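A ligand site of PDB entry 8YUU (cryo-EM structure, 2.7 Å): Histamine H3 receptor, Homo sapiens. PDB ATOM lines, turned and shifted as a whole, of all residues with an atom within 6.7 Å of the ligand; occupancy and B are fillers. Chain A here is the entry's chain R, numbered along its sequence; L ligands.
The side-chain carboxylate (OD2) of Asp 130 sits at hydrogen-bond distance from a nitrogen (N2) of the ligand (2.8 Å).
The side-chain sulfur (SG) of Cys 134 lies within hydrogen-bond range of a nitrogen (N2) of the ligand, at 3.6 Å.
A nitrogen (N3) of the ligand is in hydrogen-bond range of the backbone carbonyl oxygen of Phe 414, 2.9 Å away.
The backbone carbonyl oxygen (O) of Tyr 131 is in hydrogen-bond range of the side-chain hydroxyl (OG1) of Thr 135, 2.9 Å away.
The side-chain sulfur (SG) of Cys 134 sits at hydrogen-bond distance from the backbone carbonyl oxygen (O) of Asp 130, 3.2 Å away.
The indole nitrogen (NE1) of Trp 418 lies within hydrogen-bond range of the side-chain carboxylate (OD1) of Asp 130 (3.3 Å).
Residues that only touch the ligand: Tyr 131 (3.6 Å), Tyr 390 (3.6 Å) and Trp 418 (3.4 Å).
Hydrophobic or aromatic side chains within 4 Å of the ligand: Tyr 131, Tyr 390, Phe 414 and Trp 418.
Of the 18 residues printed, 6 come within 4 Å of the ligand.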
ATOM      1  N   VAL A  99       6.652  34.044  15.310  1.00  0.00           N
ATOM      2  CA  VAL A  99       6.780  32.822  14.524  1.00  0.00           C
ATOM      3  C   VAL A  99       8.222  32.629  14.064  1.00  0.00           C
ATOM      4  O   VAL A  99       8.733  31.510  14.040  1.00  0.00           O
ATOM      5  CB  VAL A  99       5.816  32.873  13.325  1.00  0.00           C
ATOM      6  CG1 VAL A  99       5.918  31.580  12.531  1.00  0.00           C
ATOM      7  CG2 VAL A  99       4.395  33.115  13.785  1.00  0.00           C
ATOM      8  N   TRP A 126       4.315  24.217  22.057  1.00  0.00           N
ATOM      9  CA  TRP A 126       4.693  24.601  20.693  1.00  0.00           C
ATOM     10  C   TRP A 126       3.480  24.650  19.782  1.00  0.00           C
ATOM     11  O   TRP A 126       3.342  25.583  18.986  1.00  0.00           O
ATOM     12  CB  TRP A 126       5.753  23.632  20.163  1.00  0.00           C
ATOM     13  CG  TRP A 126       6.158  23.924  18.762  1.00  0.00           C
ATOM     14  CD1 TRP A 126       6.895  24.975  18.325  1.00  0.00           C
ATOM     15  CD2 TRP A 126       5.855  23.135  17.608  1.00  0.00           C
ATOM     16  NE1 TRP A 126       7.077  24.896  16.968  1.00  0.00           N
ATOM     17  CE2 TRP A 126       6.440  23.779  16.502  1.00  0.00           C
ATOM     18  CE3 TRP A 126       5.141  21.957  17.402  1.00  0.00           C
ATOM     19  CZ2 TRP A 126       6.330  23.279  15.208  1.00  0.00           C
ATOM     20  CZ3 TRP A 126       5.034  21.464  16.114  1.00  0.00           C
ATOM     21  CH2 TRP A 126       5.631  22.121  15.035  1.00  0.00           C
ATOM     22  N   ASP A 130       2.200  27.991  17.909  1.00  0.00           N
ATOM     23  CA  ASP A 130       2.210  28.009  16.450  1.00  0.00           C
ATOM     24  C   ASP A 130       0.841  28.322  15.887  1.00  0.00           C
ATOM     25  O   ASP A 130       0.695  29.207  15.024  1.00  0.00           O
ATOM     26  CB  ASP A 130       2.709  26.646  15.933  1.00  0.00           C
ATOM     27  CG  ASP A 130       3.126  26.699  14.489  1.00  0.00           C
ATOM     28  OD1 ASP A 130       4.090  27.424  14.187  1.00  0.00           O
ATOM     29  OD2 ASP A 130       2.508  25.993  13.669  1.00  0.00           O
ATOM     30  N   TYR A 131      -0.196  27.616  16.351  1.00  0.00           N
ATOM     31  CA  TYR A 131      -1.543  27.870  15.869  1.00  0.00           C
ATOM     32  C   TYR A 131      -2.015  29.272  16.214  1.00  0.00           C
ATOM     33  O   TYR A 131      -2.630  29.938  15.371  1.00  0.00           O
ATOM     34  CB  TYR A 131      -2.512  26.828  16.425  1.00  0.00           C
ATOM     35  CG  TYR A 131      -2.429  25.506  15.715  1.00  0.00           C
ATOM     36  CD1 TYR A 131      -1.347  24.661  15.914  1.00  0.00           C
ATOM     37  CD2 TYR A 131      -3.416  25.112  14.834  1.00  0.00           C
ATOM     38  CE1 TYR A 131      -1.270  23.443  15.264  1.00  0.00           C
ATOM     39  CE2 TYR A 131      -3.340  23.894  14.184  1.00  0.00           C
ATOM     40  CZ  TYR A 131      -2.264  23.070  14.394  1.00  0.00           C
ATOM     41  OH  TYR A 131      -2.194  21.860  13.754  1.00  0.00           O
ATOM     42  N   CYS A 134      -0.244  31.714  13.727  1.00  0.00           N
ATOM     43  CA  CYS A 134      -0.762  31.648  12.355  1.00  0.00           C
ATOM     44  C   CYS A 134      -2.159  32.256  12.264  1.00  0.00           C
ATOM     45  O   CYS A 134      -2.452  33.066  11.361  1.00  0.00           O
ATOM     46  CB  CYS A 134      -0.755  30.209  11.857  1.00  0.00           C
ATOM     47  SG  CYS A 134       0.879  29.452  11.790  1.00  0.00           S
ATOM     48  N   THR A 135      -3.048  31.876  13.182  1.00  0.00           N
ATOM     49  CA  THR A 135      -4.415  32.377  13.114  1.00  0.00           C
ATOM     50  C   THR A 135      -4.471  33.878  13.389  1.00  0.00           C
ATOM     51  O   THR A 135      -5.294  34.585  12.802  1.00  0.00           O
ATOM     52  CB  THR A 135      -5.304  31.621  14.090  1.00  0.00           C
ATOM     53  OG1 THR A 135      -5.103  30.213  13.926  1.00  0.00           O
ATOM     54  CG2 THR A 135      -6.762  31.944  13.809  1.00  0.00           C
ATOM     55  N   TYR A 183      -8.290  27.422  18.301  1.00  0.00           N
ATOM     56  CA  TYR A 183      -7.510  26.186  18.224  1.00  0.00           C
ATOM     57  C   TYR A 183      -6.943  25.700  19.544  1.00  0.00           C
ATOM     58  O   TYR A 183      -6.950  24.492  19.787  1.00  0.00           O
ATOM     59  CB  TYR A 183      -6.347  26.356  17.240  1.00  0.00           C
ATOM     60  CG  TYR A 183      -6.673  25.955  15.815  1.00  0.00           C
ATOM     61  CD1 TYR A 183      -6.632  24.633  15.422  1.00  0.00           C
ATOM     62  CD2 TYR A 183      -6.997  26.916  14.860  1.00  0.00           C
ATOM     63  CE1 TYR A 183      -6.914  24.264  14.126  1.00  0.00           C
ATOM     64  CE2 TYR A 183      -7.279  26.561  13.565  1.00  0.00           C
ATOM     65  CZ  TYR A 183      -7.234  25.231  13.208  1.00  0.00           C
ATOM     66  OH  TYR A 183      -7.516  24.862  11.912  1.00  0.00           O
ATOM     67  N   PHE A 209      -5.991  15.845  12.488  1.00  0.00           N
ATOM     68  CA  PHE A 209      -5.200  15.496  11.298  1.00  0.00           C
ATOM     69  C   PHE A 209      -5.571  14.121  10.776  1.00  0.00           C
ATOM     70  O   PHE A 209      -5.016  13.695   9.751  1.00  0.00           O
ATOM     71  CB  PHE A 209      -3.691  15.526  11.568  1.00  0.00           C
ATOM     72  CG  PHE A 209      -3.112  16.899  11.705  1.00  0.00           C
ATOM     73  CD1 PHE A 209      -3.518  17.733  12.742  1.00  0.00           C
ATOM     74  CD2 PHE A 209      -2.171  17.369  10.807  1.00  0.00           C
ATOM     75  CE1 PHE A 209      -2.990  19.008  12.866  1.00  0.00           C
ATOM     76  CE2 PHE A 209      -1.640  18.637  10.938  1.00  0.00           C
ATOM     77  CZ  PHE A 209      -2.049  19.449  11.967  1.00  0.00           C
ATOM     78  N   GLU A 222     -11.094  29.759   9.639  1.00  0.00           N
ATOM     79  CA  GLU A 222      -9.752  30.312   9.756  1.00  0.00           C
ATOM     80  C   GLU A 222      -9.210  30.869   8.444  1.00  0.00           C
ATOM     81  O   GLU A 222      -8.484  31.861   8.448  1.00  0.00           O
ATOM     82  CB  GLU A 222      -8.788  29.257  10.297  1.00  0.00           C
ATOM     83  CG  GLU A 222      -7.371  29.758  10.466  1.00  0.00           C
ATOM     84  CD  GLU A 222      -6.389  28.632  10.713  1.00  0.00           C
ATOM     85  OE1 GLU A 222      -6.720  27.471  10.387  1.00  0.00           O
ATOM     86  OE2 GLU A 222      -5.282  28.904  11.234  1.00  0.00           O
ATOM     87  N   TRP A 387      -1.428  30.223   1.909  1.00  0.00           N
ATOM     88  CA  TRP A 387      -2.249  29.453   2.841  1.00  0.00           C
ATOM     89  C   TRP A 387      -3.117  28.336   2.264  1.00  0.00           C
ATOM     90  O   TRP A 387      -3.173  27.263   2.854  1.00  0.00           O
ATOM     91  CB  TRP A 387      -3.161  30.393   3.624  1.00  0.00           C
ATOM     92  CG  TRP A 387      -2.520  31.063   4.786  1.00  0.00           C
ATOM     93  CD1 TRP A 387      -1.472  31.936   4.760  1.00  0.00           C
ATOM     94  CD2 TRP A 387      -2.914  30.941   6.157  1.00  0.00           C
ATOM     95  NE1 TRP A 387      -1.176  32.348   6.036  1.00  0.00           N
ATOM     96  CE2 TRP A 387      -2.052  31.757   6.911  1.00  0.00           C
ATOM     97  CE3 TRP A 387      -3.903  30.215   6.815  1.00  0.00           C
ATOM     98  CZ2 TRP A 387      -2.156  31.863   8.298  1.00  0.00           C
ATOM     99  CZ3 TRP A 387      -4.004  30.321   8.186  1.00  0.00           C
ATOM    100  CH2 TRP A 387      -3.134  31.138   8.905  1.00  0.00           C
ATOM    101  N   TYR A 390      -1.698  24.378   1.932  1.00  0.00           N
ATOM    102  CA  TYR A 390      -1.560  23.570   3.138  1.00  0.00           C
ATOM    103  C   TYR A 390      -2.928  23.165   3.687  1.00  0.00           C
ATOM    104  O   TYR A 390      -3.123  22.014   4.101  1.00  0.00           O
ATOM    105  CB  TYR A 390      -0.767  24.339   4.194  1.00  0.00           C
ATOM    106  CG  TYR A 390      -0.861  23.723   5.571  1.00  0.00           C
ATOM    107  CD1 TYR A 390      -0.260  22.496   5.844  1.00  0.00           C
ATOM    108  CD2 TYR A 390      -1.557  24.356   6.592  1.00  0.00           C
ATOM    109  CE1 TYR A 390      -0.347  21.932   7.104  1.00  0.00           C
ATOM    110  CE2 TYR A 390      -1.634  23.792   7.848  1.00  0.00           C
ATOM    111  CZ  TYR A 390      -1.035  22.580   8.092  1.00  0.00           C
ATOM    112  OH  TYR A 390      -1.115  22.023   9.342  1.00  0.00           O
ATOM    113  N   MET A 394      -3.981  19.244   4.023  1.00  0.00           N
ATOM    114  CA  MET A 394      -4.279  18.605   5.300  1.00  0.00           C
ATOM    115  C   MET A 394      -5.682  18.043   5.323  1.00  0.00           C
ATOM    116  O   MET A 394      -5.899  16.946   5.840  1.00  0.00           O
ATOM    117  CB  MET A 394      -4.069  19.587   6.460  1.00  0.00           C
ATOM    118  CG  MET A 394      -5.237  20.529   6.706  1.00  0.00           C
ATOM    119  SD  MET A 394      -4.924  21.610   8.110  1.00  0.00           S
ATOM    120  CE  MET A 394      -6.451  22.557   8.145  1.00  0.00           C
ATOM    121  N   SER A 413       3.976  22.202   1.921  1.00  0.00           N
ATOM    122  CA  SER A 413       2.840  23.051   2.219  1.00  0.00           C
ATOM    123  C   SER A 413       2.978  23.654   3.605  1.00  0.00           C
ATOM    124  O   SER A 413       2.618  24.802   3.834  1.00  0.00           O
ATOM    125  CB  SER A 413       1.514  22.293   2.066  1.00  0.00           C
ATOM    126  OG  SER A 413       1.312  21.361   3.111  1.00  0.00           O
ATOM    127  N   PHE A 414       3.515  22.881   4.546  1.00  0.00           N
ATOM    128  CA  PHE A 414       3.708  23.349   5.912  1.00  0.00           C
ATOM    129  C   PHE A 414       4.648  24.541   5.932  1.00  0.00           C
ATOM    130  O   PHE A 414       4.398  25.514   6.639  1.00  0.00           O
ATOM    131  CB  PHE A 414       4.300  22.203   6.735  1.00  0.00           C
ATOM    132  CG  PHE A 414       4.515  22.527   8.180  1.00  0.00           C
ATOM    133  CD1 PHE A 414       5.721  23.054   8.621  1.00  0.00           C
ATOM    134  CD2 PHE A 414       3.525  22.277   9.113  1.00  0.00           C
ATOM    135  CE1 PHE A 414       5.931  23.332   9.952  1.00  0.00           C
ATOM    136  CE2 PHE A 414       3.728  22.562  10.454  1.00  0.00           C
ATOM    137  CZ  PHE A 414       4.933  23.090  10.865  1.00  0.00           C
ATOM    138  N   TRP A 415       5.724  24.483   5.161  1.00  0.00           N
ATOM    139  CA  TRP A 415       6.706  25.554   5.183  1.00  0.00           C
ATOM    140  C   TRP A 415       6.292  26.781   4.396  1.00  0.00           C
ATOM    141  O   TRP A 415       6.885  27.842   4.548  1.00  0.00           O
ATOM    142  CB  TRP A 415       8.062  25.038   4.703  1.00  0.00           C
ATOM    143  CG  TRP A 415       8.780  24.237   5.744  1.00  0.00           C
ATOM    144  CD1 TRP A 415       8.644  22.904   5.991  1.00  0.00           C
ATOM    145  CD2 TRP A 415       9.746  24.723   6.675  1.00  0.00           C
ATOM    146  NE1 TRP A 415       9.471  22.534   7.023  1.00  0.00           N
ATOM    147  CE2 TRP A 415      10.151  23.630   7.462  1.00  0.00           C
ATOM    148  CE3 TRP A 415      10.305  25.980   6.924  1.00  0.00           C
ATOM    149  CZ2 TRP A 415      11.094  23.753   8.476  1.00  0.00           C
ATOM    150  CZ3 TRP A 415      11.236  26.097   7.935  1.00  0.00           C
ATOM    151  CH2 TRP A 415      11.629  24.990   8.696  1.00  0.00           C
ATOM    152  N   LEU A 416       5.284  26.649   3.539  1.00  0.00           N
ATOM    153  CA  LEU A 416       4.762  27.793   2.779  1.00  0.00           C
ATOM    154  C   LEU A 416       4.007  28.785   3.651  1.00  0.00           C
ATOM    155  O   LEU A 416       4.103  29.983   3.440  1.00  0.00           O
ATOM    156  CB  LEU A 416       3.888  27.311   1.627  1.00  0.00           C
ATOM    157  CG  LEU A 416       3.299  28.354   0.685  1.00  0.00           C
ATOM    158  CD1 LEU A 416       4.401  29.169   0.036  1.00  0.00           C
ATOM    159  CD2 LEU A 416       2.441  27.672  -0.373  1.00  0.00           C
ATOM    160  N   LEU A 417       3.240  28.310   4.630  1.00  0.00           N
ATOM    161  CA  LEU A 417       2.557  29.228   5.547  1.00  0.00           C
ATOM    162  C   LEU A 417       3.568  30.070   6.316  1.00  0.00           C
ATOM    163  O   LEU A 417       3.326  31.258   6.544  1.00  0.00           O
ATOM    164  CB  LEU A 417       1.630  28.488   6.508  1.00  0.00           C
ATOM    165  CG  LEU A 417       0.182  28.326   6.079  1.00  0.00           C
ATOM    166  CD1 LEU A 417       0.081  27.450   4.838  1.00  0.00           C
ATOM    167  CD2 LEU A 417      -0.663  27.764   7.210  1.00  0.00           C
ATOM    168  N   TRP A 418       4.681  29.489   6.740  1.00  0.00           N
ATOM    169  CA  TRP A 418       5.733  30.247   7.428  1.00  0.00           C
ATOM    170  C   TRP A 418       6.369  31.240   6.465  1.00  0.00           C
ATOM    171  O   TRP A 418       6.660  32.358   6.853  1.00  0.00           O
ATOM    172  CB  TRP A 418       6.767  29.302   8.035  1.00  0.00           C
ATOM    173  CG  TRP A 418       6.360  28.735   9.359  1.00  0.00           C
ATOM    174  CD1 TRP A 418       5.372  29.209  10.175  1.00  0.00           C
ATOM    175  CD2 TRP A 418       6.936  27.620  10.037  1.00  0.00           C
ATOM    176  NE1 TRP A 418       5.286  28.442  11.314  1.00  0.00           N
ATOM    177  CE2 TRP A 418       6.249  27.464  11.252  1.00  0.00           C
ATOM    178  CE3 TRP A 418       7.971  26.731   9.733  1.00  0.00           C
ATOM    179  CZ2 TRP A 418       6.553  26.455  12.161  1.00  0.00           C
ATOM    180  CZ3 TRP A 418       8.285  25.736  10.638  1.00  0.00           C
ATOM    181  CH2 TRP A 418       7.572  25.602  11.842  1.00  0.00           C
HETATM  182  N1  LIG L   1      -2.263  26.288  11.594  1.00  0.00           N
HETATM  183  C1  LIG L   1      -1.184  25.525  10.976  1.00  0.00           C
HETATM  184  C2  LIG L   1       0.160  25.868  11.623  1.00  0.00           C
HETATM  185  C3  LIG L   1       1.302  25.763  10.647  1.00  0.00           C
HETATM  186  N2  LIG L   1       2.466  26.381  10.878  1.00  0.00           N
HETATM  187  C4  LIG L   1       1.411  25.123   9.464  1.00  0.00           C
HETATM  188  C5  LIG L   1       3.264  26.086   9.810  1.00  0.00           C
HETATM  189  N3  LIG L   1       2.653  25.331   8.930  1.00  0.00           N
